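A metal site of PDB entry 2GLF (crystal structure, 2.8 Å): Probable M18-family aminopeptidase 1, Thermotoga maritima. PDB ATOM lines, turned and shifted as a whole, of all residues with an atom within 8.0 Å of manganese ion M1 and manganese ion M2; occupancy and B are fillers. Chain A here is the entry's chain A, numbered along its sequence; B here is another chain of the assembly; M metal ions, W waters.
Manganese ion M2 is bound by OE2 of Glu 279 (2.0 Å), OD2 of Asp 249 (2.4 Å), NE2 of His 425 (2.4 Å) and OE1 of Glu 279 (2.6 Å). Manganese ion M2 has four donor atoms within binding distance.
Manganese ion M1 is bound by the side-chain carboxylate (OD1) of Asp 249 (2.3 Å), water W1 (2.4 Å), the side-chain carboxylate (OD2) of Asp 326 (2.4 Å), a ring nitrogen (NE2) of His 92 (2.4 Å) and the side-chain carboxylate (OD1) of Asp 326 (2.6 Å). Manganese ion M1 has five donor atoms within binding distance.
Water W1 bridges O of Val 327 (3.4 Å) and SD of Met 424 (3.5 Å).
The backbone NH of Glu 279 sits at hydrogen-bond distance from the side-chain carboxylate of Asp 94 (2.9 Å). The backbone NH (N) of Asp 249 lies within hydrogen-bond range of the side-chain carboxylate (OE1) of Glu 429, at 2.5 Å. The side-chain sulfur of Cys 253 is in hydrogen-bond range of the backbone NH of Asp 326, at 3.6 Å. A ring nitrogen (NE2) of His 425 sits close to a ring nitrogen (NE2) of His 167 of chain B (3.5 Å). The backbone NH (N) of His 425 is in hydrogen-bond range of the side-chain carboxylate (OE2) of Glu 429 (2.6 Å). The backbone carbonyl oxygen of Gly 121 is in hydrogen-bond range of a ring nitrogen (ND1) of His 425, 2.8 Å away. The backbone NH of His 92 lies within hydrogen-bond range of the side-chain carboxylate of Asp 250 (2.4 Å). A ring nitrogen (ND1) of His 92 lies within hydrogen-bond range of the side-chain carboxylate of Asp 94, at 2.9 Å.
Merely in contact with manganese ion M1: Glu 278 (3.6 Å). Of the 29 residues printed, 5 come within 4 Å of manganese ion M1.
Glu 278 touches manganese ion M2. CE of Met 424 touches manganese ion M2, at 3.4 Å.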
ATOM      1  N   ALA A  91       7.264  15.485  30.859  1.00  0.00           N
ATOM      2  CA  ALA A  91       7.965  14.696  29.853  1.00  0.00           C
ATOM      3  C   ALA A  91       8.645  13.487  30.495  1.00  0.00           C
ATOM      4  O   ALA A  91       8.622  13.321  31.714  1.00  0.00           O
ATOM      5  CB  ALA A  91       8.990  15.553  29.143  1.00  0.00           C
ATOM      6  N   HIS A  92       9.231  12.632  29.668  1.00  0.00           N
ATOM      7  CA  HIS A  92       9.931  11.456  30.173  1.00  0.00           C
ATOM      8  C   HIS A  92      11.403  11.516  29.764  1.00  0.00           C
ATOM      9  O   HIS A  92      11.741  12.036  28.705  1.00  0.00           O
ATOM     10  CB  HIS A  92       9.256  10.160  29.686  1.00  0.00           C
ATOM     11  CG  HIS A  92       9.412   9.889  28.215  1.00  0.00           C
ATOM     12  ND1 HIS A  92      10.457   9.149  27.703  1.00  0.00           N
ATOM     13  CD2 HIS A  92       8.600  10.172  27.165  1.00  0.00           C
ATOM     14  CE1 HIS A  92      10.276   8.994  26.401  1.00  0.00           C
ATOM     15  NE2 HIS A  92       9.166   9.604  26.053  1.00  0.00           N
ATOM     16  N   ASP A  94      13.478   8.658  29.956  1.00  0.00           N
ATOM     17  CA  ASP A  94      14.010   7.342  29.642  1.00  0.00           C
ATOM     18  C   ASP A  94      13.925   7.194  28.113  1.00  0.00           C
ATOM     19  O   ASP A  94      13.045   7.783  27.484  1.00  0.00           O
ATOM     20  CB  ASP A  94      13.194   6.237  30.313  1.00  0.00           C
ATOM     21  CG  ASP A  94      11.757   6.207  29.850  1.00  0.00           C
ATOM     22  OD1 ASP A  94      11.260   5.110  29.535  1.00  0.00           O
ATOM     23  OD2 ASP A  94      11.119   7.291  29.801  1.00  0.00           O
ATOM     24  N   SER A  95      14.844   6.437  27.518  1.00  0.00           N
ATOM     25  CA  SER A  95      14.852   6.233  26.072  1.00  0.00           C
ATOM     26  C   SER A  95      15.181   4.799  25.703  1.00  0.00           C
ATOM     27  O   SER A  95      15.885   4.109  26.427  1.00  0.00           O
ATOM     28  CB  SER A  95      15.882   7.145  25.417  1.00  0.00           C
ATOM     29  OG  SER A  95      15.479   8.492  25.452  1.00  0.00           O
ATOM     30  N   PRO A  96      14.658   4.322  24.555  1.00  0.00           N
ATOM     31  CA  PRO A  96      14.978   2.940  24.185  1.00  0.00           C
ATOM     32  C   PRO A  96      16.487   2.731  24.286  1.00  0.00           C
ATOM     33  O   PRO A  96      17.292   3.608  23.955  1.00  0.00           O
ATOM     34  CB  PRO A  96      14.445   2.858  22.751  1.00  0.00           C
ATOM     35  CG  PRO A  96      13.185   3.684  22.846  1.00  0.00           C
ATOM     36  CD  PRO A  96      13.661   4.904  23.631  1.00  0.00           C
ATOM     37  N   GLY A 120      12.329  -0.954  25.805  1.00  0.00           N
ATOM     38  CA  GLY A 120      11.515  -0.130  24.931  1.00  0.00           C
ATOM     39  C   GLY A 120      11.415  -0.613  23.492  1.00  0.00           C
ATOM     40  O   GLY A 120      11.867  -1.716  23.161  1.00  0.00           O
ATOM     41  N   GLY A 121      10.860   0.233  22.639  1.00  0.00           N
ATOM     42  CA  GLY A 121      10.685  -0.112  21.239  1.00  0.00           C
ATOM     43  C   GLY A 121      11.815   0.162  20.269  1.00  0.00           C
ATOM     44  O   GLY A 121      11.640   0.909  19.312  1.00  0.00           O
ATOM     45  N   GLN A 248      16.661  11.848  21.546  1.00  0.00           N
ATOM     46  CA  GLN A 248      15.930  13.097  21.426  1.00  0.00           C
ATOM     47  C   GLN A 248      14.482  12.827  21.774  1.00  0.00           C
ATOM     48  O   GLN A 248      13.733  13.743  22.102  1.00  0.00           O
ATOM     49  CB  GLN A 248      16.039  13.665  20.020  1.00  0.00           C
ATOM     50  CG  GLN A 248      17.262  14.541  19.844  1.00  0.00           C
ATOM     51  CD  GLN A 248      17.318  15.205  18.494  1.00  0.00           C
ATOM     52  OE1 GLN A 248      17.488  14.543  17.471  1.00  0.00           O
ATOM     53  NE2 GLN A 248      17.155  16.523  18.484  1.00  0.00           N
ATOM     54  N   ASP A 249      14.094  11.546  21.718  1.00  0.00           N
ATOM     55  CA  ASP A 249      12.729  11.187  22.059  1.00  0.00           C
ATOM     56  C   ASP A 249      12.491  11.592  23.502  1.00  0.00           C
ATOM     57  O   ASP A 249      12.795  10.863  24.446  1.00  0.00           O
ATOM     58  CB  ASP A 249      12.454   9.702  21.909  1.00  0.00           C
ATOM     59  CG  ASP A 249      10.970   9.356  22.094  1.00  0.00           C
ATOM     60  OD1 ASP A 249      10.301   9.972  22.946  1.00  0.00           O
ATOM     61  OD2 ASP A 249      10.469   8.448  21.400  1.00  0.00           O
ATOM     62  N   ASP A 250      11.963  12.809  23.625  1.00  0.00           N
ATOM     63  CA  ASP A 250      11.580  13.472  24.845  1.00  0.00           C
ATOM     64  C   ASP A 250      12.600  14.177  25.707  1.00  0.00           C
ATOM     65  O   ASP A 250      12.211  14.929  26.607  1.00  0.00           O
ATOM     66  CB  ASP A 250      10.741  12.556  25.710  1.00  0.00           C
ATOM     67  CG  ASP A 250       9.474  13.228  26.131  1.00  0.00           C
ATOM     68  OD1 ASP A 250       8.879  13.915  25.265  1.00  0.00           O
ATOM     69  OD2 ASP A 250       9.077  13.101  27.301  1.00  0.00           O
ATOM     70  N   ARG A 251      13.893  13.959  25.494  1.00  0.00           N
ATOM     71  CA  ARG A 251      14.839  14.722  26.287  1.00  0.00           C
ATOM     72  C   ARG A 251      14.831  16.088  25.617  1.00  0.00           C
ATOM     73  O   ARG A 251      15.270  17.084  26.189  1.00  0.00           O
ATOM     74  CB  ARG A 251      16.246  14.102  26.267  1.00  0.00           C
ATOM     75  CG  ARG A 251      16.274  12.695  26.836  1.00  0.00           C
ATOM     76  CD  ARG A 251      17.593  12.344  27.502  1.00  0.00           C
ATOM     77  NE  ARG A 251      17.465  11.073  28.210  1.00  0.00           N
ATOM     78  CZ  ARG A 251      17.762   9.883  27.699  1.00  0.00           C
ATOM     79  NH1 ARG A 251      18.226   9.789  26.467  1.00  0.00           N
ATOM     80  NH2 ARG A 251      17.581   8.786  28.419  1.00  0.00           N
ATOM     81  N   CYS A 253      12.062  17.445  24.799  1.00  0.00           N
ATOM     82  CA  CYS A 253      10.937  18.095  25.440  1.00  0.00           C
ATOM     83  C   CYS A 253      11.295  18.395  26.881  1.00  0.00           C
ATOM     84  O   CYS A 253      10.780  19.343  27.470  1.00  0.00           O
ATOM     85  CB  CYS A 253       9.697  17.221  25.378  1.00  0.00           C
ATOM     86  SG  CYS A 253       8.888  17.387  23.815  1.00  0.00           S
ATOM     87  N   GLU A 278       8.496   5.506  30.828  1.00  0.00           N
ATOM     88  CA  GLU A 278       7.396   5.739  29.895  1.00  0.00           C
ATOM     89  C   GLU A 278       7.506   4.796  28.700  1.00  0.00           C
ATOM     90  O   GLU A 278       6.499   4.243  28.246  1.00  0.00           O
ATOM     91  CB  GLU A 278       7.388   7.185  29.387  1.00  0.00           C
ATOM     92  CG  GLU A 278       7.731   7.321  27.914  1.00  0.00           C
ATOM     93  CD  GLU A 278       6.576   7.049  26.988  1.00  0.00           C
ATOM     94  OE1 GLU A 278       6.803   7.003  25.755  1.00  0.00           O
ATOM     95  OE2 GLU A 278       5.435   6.903  27.478  1.00  0.00           O
ATOM     96  N   GLU A 279       8.728   4.626  28.197  1.00  0.00           N
ATOM     97  CA  GLU A 279       8.979   3.762  27.045  1.00  0.00           C
ATOM     98  C   GLU A 279       8.572   2.300  27.250  1.00  0.00           C
ATOM     99  O   GLU A 279       8.709   1.501  26.332  1.00  0.00           O
ATOM    100  CB  GLU A 279      10.464   3.819  26.647  1.00  0.00           C
ATOM    101  CG  GLU A 279      10.950   5.128  26.040  1.00  0.00           C
ATOM    102  CD  GLU A 279      10.308   5.464  24.702  1.00  0.00           C
ATOM    103  OE1 GLU A 279       9.575   4.632  24.148  1.00  0.00           O
ATOM    104  OE2 GLU A 279      10.529   6.578  24.198  1.00  0.00           O
ATOM    105  N   ILE A 280       8.111   1.941  28.450  1.00  0.00           N
ATOM    106  CA  ILE A 280       7.681   0.566  28.699  1.00  0.00           C
ATOM    107  C   ILE A 280       6.274   0.512  29.301  1.00  0.00           C
ATOM    108  O   ILE A 280       5.838  -0.535  29.780  1.00  0.00           O
ATOM    109  CB  ILE A 280       8.672  -0.220  29.637  1.00  0.00           C
ATOM    110  CG1 ILE A 280       8.923   0.516  30.953  1.00  0.00           C
ATOM    111  CG2 ILE A 280       9.980  -0.460  28.907  1.00  0.00           C
ATOM    112  CD1 ILE A 280       7.815   0.343  31.999  1.00  0.00           C
ATOM    113  N   GLY A 325       4.435  16.979  27.222  1.00  0.00           N
ATOM    114  CA  GLY A 325       5.531  17.243  26.310  1.00  0.00           C
ATOM    115  C   GLY A 325       6.220  16.019  25.744  1.00  0.00           C
ATOM    116  O   GLY A 325       7.113  15.443  26.379  1.00  0.00           O
ATOM    117  N   ASP A 326       5.821  15.614  24.538  1.00  0.00           N
ATOM    118  CA  ASP A 326       6.411  14.459  23.872  1.00  0.00           C
ATOM    119  C   ASP A 326       6.466  14.735  22.365  1.00  0.00           C
ATOM    120  O   ASP A 326       5.726  15.575  21.850  1.00  0.00           O
ATOM    121  CB  ASP A 326       5.621  13.193  24.166  1.00  0.00           C
ATOM    122  CG  ASP A 326       6.470  11.933  24.054  1.00  0.00           C
ATOM    123  OD1 ASP A 326       6.005  10.859  24.498  1.00  0.00           O
ATOM    124  OD2 ASP A 326       7.598  12.006  23.533  1.00  0.00           O
ATOM    125  N   VAL A 327       7.331  14.022  21.664  1.00  0.00           N
ATOM    126  CA  VAL A 327       7.525  14.206  20.229  1.00  0.00           C
ATOM    127  C   VAL A 327       6.546  13.461  19.343  1.00  0.00           C
ATOM    128  O   VAL A 327       5.990  12.438  19.735  1.00  0.00           O
ATOM    129  CB  VAL A 327       8.938  13.745  19.809  1.00  0.00           C
ATOM    130  CG1 VAL A 327      10.000  14.509  20.591  1.00  0.00           C
ATOM    131  CG2 VAL A 327       9.069  12.253  20.060  1.00  0.00           C
ATOM    132  N   CYS A 328       6.329  13.988  18.141  1.00  0.00           N
ATOM    133  CA  CYS A 328       5.445  13.335  17.182  1.00  0.00           C
ATOM    134  C   CYS A 328       6.316  12.990  15.982  1.00  0.00           C
ATOM    135  O   CYS A 328       7.521  13.260  15.980  1.00  0.00           O
ATOM    136  CB  CYS A 328       4.312  14.277  16.761  1.00  0.00           C
ATOM    137  SG  CYS A 328       4.879  15.850  16.085  1.00  0.00           S
ATOM    138  N   GLY A 400       0.327   4.792  19.483  1.00  0.00           N
ATOM    139  CA  GLY A 400       1.172   5.762  20.135  1.00  0.00           C
ATOM    140  C   GLY A 400       0.999   5.714  21.638  1.00  0.00           C
ATOM    141  O   GLY A 400       1.676   4.942  22.315  1.00  0.00           O
ATOM    142  N   GLY A 401       0.072   6.517  22.153  1.00  0.00           N
ATOM    143  CA  GLY A 401      -0.168   6.539  23.581  1.00  0.00           C
ATOM    144  C   GLY A 401       0.965   7.203  24.339  1.00  0.00           C
ATOM    145  O   GLY A 401       2.092   6.697  24.352  1.00  0.00           O
ATOM    146  N   THR A 402       0.679   8.339  24.969  1.00  0.00           N
ATOM    147  CA  THR A 402       1.678   9.059  25.750  1.00  0.00           C
ATOM    148  C   THR A 402       1.237   9.066  27.208  1.00  0.00           C
ATOM    149  O   THR A 402       0.211   8.481  27.541  1.00  0.00           O
ATOM    150  CB  THR A 402       1.829  10.512  25.280  1.00  0.00           C
ATOM    151  OG1 THR A 402       0.569  11.173  25.384  1.00  0.00           O
ATOM    152  CG2 THR A 402       2.322  10.577  23.845  1.00  0.00           C
ATOM    153  N   ILE A 403       2.003   9.737  28.056  1.00  0.00           N
ATOM    154  CA  ILE A 403       1.664   9.784  29.474  1.00  0.00           C
ATOM    155  C   ILE A 403       0.535  10.747  29.809  1.00  0.00           C
ATOM    156  O   ILE A 403       0.062  10.795  30.946  1.00  0.00           O
ATOM    157  CB  ILE A 403       2.901  10.129  30.329  1.00  0.00           C
ATOM    158  CG1 ILE A 403       3.292  11.597  30.146  1.00  0.00           C
ATOM    159  CG2 ILE A 403       4.061   9.237  29.939  1.00  0.00           C
ATOM    160  CD1 ILE A 403       4.392  12.051  31.098  1.00  0.00           C
ATOM    161  N   LEU A 421       9.763  14.533  14.885  1.00  0.00           N
ATOM    162  CA  LEU A 421      11.059  13.893  14.641  1.00  0.00           C
ATOM    163  C   LEU A 421      11.060  12.923  13.469  1.00  0.00           C
ATOM    164  O   LEU A 421      10.038  12.360  13.097  1.00  0.00           O
ATOM    165  CB  LEU A 421      11.541  13.118  15.874  1.00  0.00           C
ATOM    166  CG  LEU A 421      11.756  13.767  17.228  1.00  0.00           C
ATOM    167  CD1 LEU A 421      12.347  12.737  18.151  1.00  0.00           C
ATOM    168  CD2 LEU A 421      12.686  14.960  17.112  1.00  0.00           C
ATOM    169  N   MET A 424      12.338   8.342  14.700  1.00  0.00           N
ATOM    170  CA  MET A 424      12.119   8.207  16.142  1.00  0.00           C
ATOM    171  C   MET A 424      12.552   6.803  16.585  1.00  0.00           C
ATOM    172  O   MET A 424      12.333   5.827  15.878  1.00  0.00           O
ATOM    173  CB  MET A 424      10.655   8.455  16.472  1.00  0.00           C
ATOM    174  CG  MET A 424      10.382   8.777  17.942  1.00  0.00           C
ATOM    175  SD  MET A 424       8.496   9.141  18.304  1.00  0.00           S
ATOM    176  CE  MET A 424       8.137   7.761  19.618  1.00  0.00           C
ATOM    177  N   HIS A 425      13.178   6.723  17.755  1.00  0.00           N
ATOM    178  CA  HIS A 425      13.681   5.473  18.343  1.00  0.00           C
ATOM    179  C   HIS A 425      14.955   4.913  17.740  1.00  0.00           C
ATOM    180  O   HIS A 425      15.508   3.939  18.259  1.00  0.00           O
ATOM    181  CB  HIS A 425      12.601   4.391  18.340  1.00  0.00           C
ATOM    182  CG  HIS A 425      11.574   4.570  19.405  1.00  0.00           C
ATOM    183  ND1 HIS A 425      10.785   3.545  19.862  1.00  0.00           N
ATOM    184  CD2 HIS A 425      11.218   5.659  20.118  1.00  0.00           C
ATOM    185  CE1 HIS A 425       9.999   3.987  20.817  1.00  0.00           C
ATOM    186  NE2 HIS A 425      10.238   5.276  20.992  1.00  0.00           N
ATOM    187  N   GLU A 429      18.205  10.078  16.113  1.00  0.00           N
ATOM    188  CA  GLU A 429      16.988  10.777  15.727  1.00  0.00           C
ATOM    189  C   GLU A 429      17.300  12.161  15.179  1.00  0.00           C
ATOM    190  O   GLU A 429      18.336  12.745  15.485  1.00  0.00           O
ATOM    191  CB  GLU A 429      16.042  10.888  16.923  1.00  0.00           C
ATOM    192  CG  GLU A 429      15.733   9.543  17.564  1.00  0.00           C
ATOM    193  CD  GLU A 429      14.888   9.664  18.816  1.00  0.00           C
ATOM    194  OE1 GLU A 429      15.154  10.567  19.639  1.00  0.00           O
ATOM    195  OE2 GLU A 429      13.960   8.839  19.007  1.00  0.00           O
ATOM    196  N   PRO B 166       9.415   2.977  14.293  1.00  0.00           N
ATOM    197  CA  PRO B 166       8.762   1.676  14.401  1.00  0.00           C
ATOM    198  C   PRO B 166       7.262   1.712  14.696  1.00  0.00           C
ATOM    199  O   PRO B 166       6.575   0.715  14.512  1.00  0.00           O
ATOM    200  CB  PRO B 166       9.565   0.993  15.515  1.00  0.00           C
ATOM    201  CG  PRO B 166      10.011   2.142  16.356  1.00  0.00           C
ATOM    202  CD  PRO B 166      10.441   3.150  15.341  1.00  0.00           C
ATOM    203  N   HIS B 167       6.755   2.865  15.119  1.00  0.00           N
ATOM    204  CA  HIS B 167       5.339   3.029  15.440  1.00  0.00           C
ATOM    205  C   HIS B 167       4.422   3.021  14.231  1.00  0.00           C
ATOM    206  O   HIS B 167       3.246   2.675  14.334  1.00  0.00           O
ATOM    207  CB  HIS B 167       5.111   4.351  16.173  1.00  0.00           C
ATOM    208  CG  HIS B 167       6.099   4.610  17.263  1.00  0.00           C
ATOM    209  ND1 HIS B 167       5.884   4.230  18.573  1.00  0.00           N
ATOM    210  CD2 HIS B 167       7.329   5.160  17.237  1.00  0.00           C
ATOM    211  CE1 HIS B 167       6.937   4.547  19.303  1.00  0.00           C
ATOM    212  NE2 HIS B 167       7.827   5.116  18.518  1.00  0.00           N
HETATM  213 MN    MN M   1       8.177   9.700  23.818  1.00  0.00          MN
HETATM  214 MN    MN M   2       9.251   6.766  22.625  1.00  0.00          MN
HETATM  215  O   HOH W   1       7.614  10.133  21.563  1.00  0.00           O
